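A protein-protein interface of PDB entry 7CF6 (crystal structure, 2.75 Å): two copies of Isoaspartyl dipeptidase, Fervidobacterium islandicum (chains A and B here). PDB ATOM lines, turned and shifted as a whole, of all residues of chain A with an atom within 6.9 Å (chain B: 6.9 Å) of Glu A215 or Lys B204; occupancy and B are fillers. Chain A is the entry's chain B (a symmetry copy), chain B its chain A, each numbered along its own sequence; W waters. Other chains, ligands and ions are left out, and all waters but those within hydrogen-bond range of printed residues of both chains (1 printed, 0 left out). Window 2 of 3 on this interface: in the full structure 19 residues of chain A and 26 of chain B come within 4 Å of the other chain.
Among the printed residues, 7 pairs touch across the chains.
Among the printed residues, merely in contact across the chains: Glu A218 with Ser B164 (3.2 Å), Thr A217 with Arg B205 (3.6 Å), Lys A216 with Arg B205 (3.6 Å), Thr A217 with Lys B204 (3.6 Å), Glu A215 with Lys B204 (3.8 Å) and Glu A218 with Gly B203 (3.8 Å).
Water W1 lies within hydrogen-bond range of the backbone carbonyl oxygen (O) of Glu A215 (2.8 Å), the backbone carbonyl oxygen (O) of Ile A214 (3.0 Å) and the side-chain amino group (NZ) of Lys B204 (3.1 Å).
The side-chain carboxylate of Glu A218 lies within salt-bridge range of the guanidinium group of Arg B205 (3.3 Å).
Glu A215 touches just one residue of chain B: Lys B204. Of the printed residues of chain B, Lys A216 touches Arg B205. Printed residues of chain B within 4 Å of Thr A217: Lys B204 (3.6 Å) and Arg B205 (3.6 Å). Of the printed residues of chain B, Glu A218 touches Ser B164 (3.2 Å), Gly B203 (3.8 Å) and Arg B205 (3.3 Å). Of the printed residues of chain A, Gly B203 touches Glu A218. Of chain A, only Glu A215 and Thr A217 come within 4 Å of Lys B204. Printed residues of chain A within 4 Å of Arg B205: Lys A216 (3.6 Å), Thr A217 (3.6 Å) and Glu A218 (3.3 Å). Gly B206 touches none of the printed residues of chain A. Glu B208 touches none of the printed residues of chain A. The nearest residue of chain A that does not touch Lys B204 is Lys A216 (4.4 Å).
The backbone carbonyl oxygen of Ser B164 is in hydrogen-bond range of the backbone NH of Ser B202. The backbone carbonyl oxygen (O) of Ser B164 is in hydrogen-bond range of the backbone NH (N) of Gly B203 (3.1 Å). OG of Ser B164 is in hydrogen-bond range of O of Gly B206, at 2.7 Å. O of Ile A213 lies within hydrogen-bond range of OG1 of Thr A217 (2.5 Å). The guanidinium group (NH2) of Arg A245 lies within salt-bridge range of the side-chain carboxylate (OE1) of Glu A215 (2.9 Å).
1 position is printed for both chains. Of the 7 pairs that touch across the chains among the printed residues, none has its exchanged pair printed and touching as well.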
ATOM      1  N   GLU A 208     -22.681   9.515 -18.930  1.00  0.00           N
ATOM      2  CA  GLU A 208     -21.546   9.718 -19.870  1.00  0.00           C
ATOM      3  C   GLU A 208     -20.366   8.861 -19.418  1.00  0.00           C
ATOM      4  O   GLU A 208     -19.887   8.066 -20.231  1.00  0.00           O
ATOM      5  CB  GLU A 208     -21.122  11.181 -19.923  1.00  0.00           C
ATOM      6  CG  GLU A 208     -21.735  11.921 -21.090  1.00  0.00           C
ATOM      7  CD  GLU A 208     -21.478  13.420 -21.082  1.00  0.00           C
ATOM      8  OE1 GLU A 208     -22.210  14.140 -21.822  1.00  0.00           O
ATOM      9  OE2 GLU A 208     -20.562  13.866 -20.324  1.00  0.00           O
ATOM     10  N   TYR A 209     -19.958   9.020 -18.155  1.00  0.00           N
ATOM     11  CA  TYR A 209     -18.785   8.353 -17.534  1.00  0.00           C
ATOM     12  C   TYR A 209     -18.818   6.852 -17.812  1.00  0.00           C
ATOM     13  O   TYR A 209     -17.791   6.307 -18.253  1.00  0.00           O
ATOM     14  CB  TYR A 209     -18.767   8.636 -16.035  1.00  0.00           C
ATOM     15  CG  TYR A 209     -18.074   9.910 -15.647  1.00  0.00           C
ATOM     16  CD1 TYR A 209     -17.253  10.581 -16.532  1.00  0.00           C
ATOM     17  CD2 TYR A 209     -18.200  10.416 -14.373  1.00  0.00           C
ATOM     18  CE1 TYR A 209     -16.593  11.736 -16.175  1.00  0.00           C
ATOM     19  CE2 TYR A 209     -17.543  11.570 -13.995  1.00  0.00           C
ATOM     20  CZ  TYR A 209     -16.724  12.216 -14.894  1.00  0.00           C
ATOM     21  OH  TYR A 209     -16.051  13.333 -14.523  1.00  0.00           O
ATOM     22  N   LEU A 210     -19.965   6.208 -17.580  1.00  0.00           N
ATOM     23  CA  LEU A 210     -20.124   4.729 -17.695  1.00  0.00           C
ATOM     24  C   LEU A 210     -19.735   4.292 -19.112  1.00  0.00           C
ATOM     25  O   LEU A 210     -19.148   3.237 -19.240  1.00  0.00           O
ATOM     26  CB  LEU A 210     -21.572   4.322 -17.376  1.00  0.00           C
ATOM     27  CG  LEU A 210     -21.935   4.164 -15.898  1.00  0.00           C
ATOM     28  CD1 LEU A 210     -21.804   5.470 -15.125  1.00  0.00           C
ATOM     29  CD2 LEU A 210     -23.348   3.628 -15.775  1.00  0.00           C
ATOM     30  N   PHE A 211     -20.081   5.096 -20.118  1.00  0.00           N
ATOM     31  CA  PHE A 211     -19.778   4.888 -21.561  1.00  0.00           C
ATOM     32  C   PHE A 211     -18.294   5.155 -21.877  1.00  0.00           C
ATOM     33  O   PHE A 211     -17.708   4.418 -22.700  1.00  0.00           O
ATOM     34  CB  PHE A 211     -20.667   5.808 -22.395  1.00  0.00           C
ATOM     35  CG  PHE A 211     -22.112   5.387 -22.460  1.00  0.00           C
ATOM     36  CD1 PHE A 211     -22.485   4.242 -23.144  1.00  0.00           C
ATOM     37  CD2 PHE A 211     -23.105   6.183 -21.927  1.00  0.00           C
ATOM     38  CE1 PHE A 211     -23.817   3.877 -23.251  1.00  0.00           C
ATOM     39  CE2 PHE A 211     -24.437   5.811 -22.028  1.00  0.00           C
ATOM     40  CZ  PHE A 211     -24.789   4.653 -22.679  1.00  0.00           C
ATOM     41  N   ASP A 212     -17.704   6.177 -21.246  1.00  0.00           N
ATOM     42  CA  ASP A 212     -16.235   6.437 -21.252  1.00  0.00           C
ATOM     43  C   ASP A 212     -15.494   5.205 -20.711  1.00  0.00           C
ATOM     44  O   ASP A 212     -14.520   4.805 -21.366  1.00  0.00           O
ATOM     45  CB  ASP A 212     -15.847   7.691 -20.451  1.00  0.00           C
ATOM     46  CG  ASP A 212     -16.375   9.008 -21.005  1.00  0.00           C
ATOM     47  OD1 ASP A 212     -16.532   9.118 -22.231  1.00  0.00           O
ATOM     48  OD2 ASP A 212     -16.643   9.915 -20.198  1.00  0.00           O
ATOM     49  N   ILE A 213     -15.937   4.621 -19.583  1.00  0.00           N
ATOM     50  CA  ILE A 213     -15.248   3.459 -18.938  1.00  0.00           C
ATOM     51  C   ILE A 213     -15.166   2.282 -19.922  1.00  0.00           C
ATOM     52  O   ILE A 213     -14.100   1.663 -20.000  1.00  0.00           O
ATOM     53  CB  ILE A 213     -15.922   3.030 -17.623  1.00  0.00           C
ATOM     54  CG1 ILE A 213     -15.779   4.083 -16.522  1.00  0.00           C
ATOM     55  CG2 ILE A 213     -15.358   1.690 -17.165  1.00  0.00           C
ATOM     56  CD1 ILE A 213     -16.637   3.815 -15.287  1.00  0.00           C
ATOM     57  N   ILE A 214     -16.251   1.954 -20.619  1.00  0.00           N
ATOM     58  CA  ILE A 214     -16.360   0.719 -21.460  1.00  0.00           C
ATOM     59  C   ILE A 214     -15.724   0.942 -22.849  1.00  0.00           C
ATOM     60  O   ILE A 214     -15.427  -0.081 -23.520  1.00  0.00           O
ATOM     61  CB  ILE A 214     -17.827   0.250 -21.573  1.00  0.00           C
ATOM     62  CG1 ILE A 214     -18.700   1.300 -22.269  1.00  0.00           C
ATOM     63  CG2 ILE A 214     -18.375  -0.145 -20.203  1.00  0.00           C
ATOM     64  CD1 ILE A 214     -20.105   0.844 -22.581  1.00  0.00           C
ATOM     65  N   GLU A 215     -15.544   2.203 -23.280  1.00  0.00           N
ATOM     66  CA  GLU A 215     -15.003   2.555 -24.627  1.00  0.00           C
ATOM     67  C   GLU A 215     -13.480   2.746 -24.526  1.00  0.00           C
ATOM     68  O   GLU A 215     -12.785   2.391 -25.479  1.00  0.00           O
ATOM     69  CB  GLU A 215     -15.670   3.811 -25.212  1.00  0.00           C
ATOM     70  CG  GLU A 215     -17.044   3.580 -25.840  1.00  0.00           C
ATOM     71  CD  GLU A 215     -17.783   4.864 -26.213  1.00  0.00           C
ATOM     72  OE1 GLU A 215     -18.958   5.069 -25.804  1.00  0.00           O
ATOM     73  OE2 GLU A 215     -17.180   5.659 -26.913  1.00  0.00           O
ATOM     74  N   LYS A 216     -12.953   3.214 -23.398  1.00  0.00           N
ATOM     75  CA  LYS A 216     -11.518   3.595 -23.309  1.00  0.00           C
ATOM     76  C   LYS A 216     -10.629   2.508 -22.662  1.00  0.00           C
ATOM     77  O   LYS A 216      -9.389   2.591 -22.883  1.00  0.00           O
ATOM     78  CB  LYS A 216     -11.399   4.947 -22.599  1.00  0.00           C
ATOM     79  CG  LYS A 216     -12.072   6.078 -23.347  1.00  0.00           C
ATOM     80  CD  LYS A 216     -12.119   7.372 -22.596  1.00  0.00           C
ATOM     81  CE  LYS A 216     -12.605   8.516 -23.471  1.00  0.00           C
ATOM     82  NZ  LYS A 216     -12.344   9.843 -22.853  1.00  0.00           N
ATOM     83  N   THR A 217     -11.180   1.550 -21.904  1.00  0.00           N
ATOM     84  CA  THR A 217     -10.401   0.687 -20.969  1.00  0.00           C
ATOM     85  C   THR A 217     -10.792  -0.775 -21.170  1.00  0.00           C
ATOM     86  O   THR A 217     -11.674  -1.008 -22.008  1.00  0.00           O
ATOM     87  CB  THR A 217     -10.628   1.102 -19.513  1.00  0.00           C
ATOM     88  OG1 THR A 217     -11.960   0.730 -19.175  1.00  0.00           O
ATOM     89  CG2 THR A 217     -10.445   2.582 -19.283  1.00  0.00           C
ATOM     90  N   GLU A 218     -10.158  -1.703 -20.437  1.00  0.00           N
ATOM     91  CA  GLU A 218     -10.370  -3.178 -20.590  1.00  0.00           C
ATOM     92  C   GLU A 218     -11.474  -3.655 -19.626  1.00  0.00           C
ATOM     93  O   GLU A 218     -11.815  -4.856 -19.702  1.00  0.00           O
ATOM     94  CB  GLU A 218      -9.073  -3.976 -20.354  1.00  0.00           C
ATOM     95  CG  GLU A 218      -7.848  -3.482 -21.130  1.00  0.00           C
ATOM     96  CD  GLU A 218      -7.087  -2.264 -20.591  1.00  0.00           C
ATOM     97  OE1 GLU A 218      -6.212  -1.753 -21.326  1.00  0.00           O
ATOM     98  OE2 GLU A 218      -7.363  -1.808 -19.452  1.00  0.00           O
ATOM     99  N   ILE A 219     -12.005  -2.762 -18.773  1.00  0.00           N
ATOM    100  CA  ILE A 219     -12.876  -3.134 -17.619  1.00  0.00           C
ATOM    101  C   ILE A 219     -14.227  -3.629 -18.132  1.00  0.00           C
ATOM    102  O   ILE A 219     -14.939  -2.917 -18.828  1.00  0.00           O
ATOM    103  CB  ILE A 219     -13.057  -1.976 -16.618  1.00  0.00           C
ATOM    104  CG1 ILE A 219     -11.731  -1.523 -15.998  1.00  0.00           C
ATOM    105  CG2 ILE A 219     -14.087  -2.366 -15.548  1.00  0.00           C
ATOM    106  CD1 ILE A 219     -11.872  -0.397 -14.995  1.00  0.00           C
ATOM    107  N   ARG A 245     -25.718  -2.500 -25.054  1.00  0.00           N
ATOM    108  CA  ARG A 245     -24.268  -2.840 -25.070  1.00  0.00           C
ATOM    109  C   ARG A 245     -23.981  -4.034 -24.156  1.00  0.00           C
ATOM    110  O   ARG A 245     -22.836  -4.439 -24.128  1.00  0.00           O
ATOM    111  CB  ARG A 245     -23.420  -1.640 -24.627  1.00  0.00           C
ATOM    112  CG  ARG A 245     -23.621  -0.376 -25.461  1.00  0.00           C
ATOM    113  CD  ARG A 245     -22.696  -0.265 -26.669  1.00  0.00           C
ATOM    114  NE  ARG A 245     -21.561   0.643 -26.454  1.00  0.00           N
ATOM    115  CZ  ARG A 245     -21.575   1.980 -26.609  1.00  0.00           C
ATOM    116  NH1 ARG A 245     -22.682   2.607 -26.990  1.00  0.00           N
ATOM    117  NH2 ARG A 245     -20.468   2.678 -26.378  1.00  0.00           N
ATOM    118  N   SER B 164      -2.516  -2.316 -19.690  1.00  0.00           N
ATOM    119  CA  SER B 164      -3.285  -2.919 -20.806  1.00  0.00           C
ATOM    120  C   SER B 164      -3.848  -4.267 -20.346  1.00  0.00           C
ATOM    121  O   SER B 164      -3.671  -5.280 -21.090  1.00  0.00           O
ATOM    122  CB  SER B 164      -2.446  -3.084 -22.068  1.00  0.00           C
ATOM    123  OG  SER B 164      -2.141  -1.828 -22.639  1.00  0.00           O
ATOM    124  N   SER B 202      -3.852  -7.709 -22.805  1.00  0.00           N
ATOM    125  CA  SER B 202      -4.329  -7.849 -24.200  1.00  0.00           C
ATOM    126  C   SER B 202      -5.204  -6.639 -24.559  1.00  0.00           C
ATOM    127  O   SER B 202      -6.054  -6.751 -25.452  1.00  0.00           O
ATOM    128  CB  SER B 202      -5.035  -9.170 -24.343  1.00  0.00           C
ATOM    129  OG  SER B 202      -5.399  -9.662 -23.064  1.00  0.00           O
ATOM    130  N   GLY B 203      -4.984  -5.507 -23.884  1.00  0.00           N
ATOM    131  CA  GLY B 203      -5.626  -4.221 -24.213  1.00  0.00           C
ATOM    132  C   GLY B 203      -5.163  -3.743 -25.574  1.00  0.00           C
ATOM    133  O   GLY B 203      -4.060  -4.130 -25.996  1.00  0.00           O
ATOM    134  N   LYS B 204      -5.994  -2.966 -26.260  1.00  0.00           N
ATOM    135  CA  LYS B 204      -5.645  -2.280 -27.532  1.00  0.00           C
ATOM    136  C   LYS B 204      -4.438  -1.345 -27.311  1.00  0.00           C
ATOM    137  O   LYS B 204      -3.686  -1.150 -28.259  1.00  0.00           O
ATOM    138  CB  LYS B 204      -6.876  -1.553 -28.104  1.00  0.00           C
ATOM    139  CG  LYS B 204      -7.632  -0.618 -27.153  1.00  0.00           C
ATOM    140  CD  LYS B 204      -9.131  -0.436 -27.466  1.00  0.00           C
ATOM    141  CE  LYS B 204     -10.004  -0.107 -26.261  1.00  0.00           C
ATOM    142  NZ  LYS B 204     -10.042  -1.207 -25.260  1.00  0.00           N
ATOM    143  N   ARG B 205      -4.224  -0.797 -26.113  1.00  0.00           N
ATOM    144  CA  ARG B 205      -3.176   0.238 -25.887  1.00  0.00           C
ATOM    145  C   ARG B 205      -1.755  -0.350 -25.923  1.00  0.00           C
ATOM    146  O   ARG B 205      -0.812   0.446 -25.926  1.00  0.00           O
ATOM    147  CB  ARG B 205      -3.416   0.938 -24.550  1.00  0.00           C
ATOM    148  CG  ARG B 205      -4.690   1.764 -24.526  1.00  0.00           C
ATOM    149  CD  ARG B 205      -4.887   2.451 -23.196  1.00  0.00           C
ATOM    150  NE  ARG B 205      -5.678   1.653 -22.280  1.00  0.00           N
ATOM    151  CZ  ARG B 205      -6.229   2.142 -21.175  1.00  0.00           C
ATOM    152  NH1 ARG B 205      -6.052   3.414 -20.851  1.00  0.00           N
ATOM    153  NH2 ARG B 205      -6.947   1.362 -20.385  1.00  0.00           N
ATOM    154  N   GLY B 206      -1.607  -1.679 -25.882  1.00  0.00           N
ATOM    155  CA  GLY B 206      -0.321  -2.415 -25.873  1.00  0.00           C
ATOM    156  C   GLY B 206       0.673  -1.834 -24.884  1.00  0.00           C
ATOM    157  O   GLY B 206       0.356  -1.761 -23.683  1.00  0.00           O
ATOM    158  N   ILE B 207       1.839  -1.414 -25.369  1.00  0.00           N
ATOM    159  CA  ILE B 207       2.907  -0.803 -24.526  1.00  0.00           C
ATOM    160  C   ILE B 207       3.032   0.685 -24.880  1.00  0.00           C
ATOM    161  O   ILE B 207       4.118   1.261 -24.674  1.00  0.00           O
ATOM    162  CB  ILE B 207       4.251  -1.559 -24.662  1.00  0.00           C
ATOM    163  CG1 ILE B 207       4.675  -1.725 -26.120  1.00  0.00           C
ATOM    164  CG2 ILE B 207       4.219  -2.899 -23.938  1.00  0.00           C
ATOM    165  CD1 ILE B 207       6.167  -1.899 -26.295  1.00  0.00           C
ATOM    166  N   GLU B 208       1.959   1.313 -25.353  1.00  0.00           N
ATOM    167  CA  GLU B 208       1.989   2.751 -25.739  1.00  0.00           C
ATOM    168  C   GLU B 208       2.755   3.577 -24.696  1.00  0.00           C
ATOM    169  O   GLU B 208       3.495   4.489 -25.099  1.00  0.00           O
ATOM    170  CB  GLU B 208       0.580   3.315 -25.890  1.00  0.00           C
ATOM    171  CG  GLU B 208       0.098   3.306 -27.322  1.00  0.00           C
ATOM    172  CD  GLU B 208      -1.400   3.479 -27.437  1.00  0.00           C
ATOM    173  OE1 GLU B 208      -1.972   2.908 -28.396  1.00  0.00           O
ATOM    174  OE2 GLU B 208      -1.982   4.159 -26.544  1.00  0.00           O
ATOM    175  N   LYS B 234       0.336  -9.218 -32.893  1.00  0.00           N
ATOM    176  CA  LYS B 234       0.235  -7.739 -32.868  1.00  0.00           C
ATOM    177  C   LYS B 234       1.193  -7.218 -31.792  1.00  0.00           C
ATOM    178  O   LYS B 234       1.937  -6.261 -32.060  1.00  0.00           O
ATOM    179  CB  LYS B 234      -1.213  -7.306 -32.624  1.00  0.00           C
ATOM    180  CG  LYS B 234      -1.508  -5.878 -33.051  1.00  0.00           C
ATOM    181  CD  LYS B 234      -2.852  -5.370 -32.583  1.00  0.00           C
ATOM    182  CE  LYS B 234      -2.974  -3.865 -32.703  1.00  0.00           C
ATOM    183  NZ  LYS B 234      -4.313  -3.389 -32.295  1.00  0.00           N
ATOM    184  N   GLN B 238       4.948  -5.088 -32.037  1.00  0.00           N
ATOM    185  CA  GLN B 238       5.216  -3.887 -31.177  1.00  0.00           C
ATOM    186  C   GLN B 238       6.505  -4.092 -30.354  1.00  0.00           C
ATOM    187  O   GLN B 238       7.183  -3.067 -30.017  1.00  0.00           O
ATOM    188  CB  GLN B 238       4.041  -3.586 -30.230  1.00  0.00           C
ATOM    189  CG  GLN B 238       3.161  -2.413 -30.670  1.00  0.00           C
ATOM    190  CD  GLN B 238       2.571  -1.599 -29.533  1.00  0.00           C
ATOM    191  OE1 GLN B 238       1.950  -2.107 -28.600  1.00  0.00           O
ATOM    192  NE2 GLN B 238       2.725  -0.290 -29.627  1.00  0.00           N
HETATM  193  O   HOH W   1     -13.014  -0.424 -25.321  1.00  0.00           O
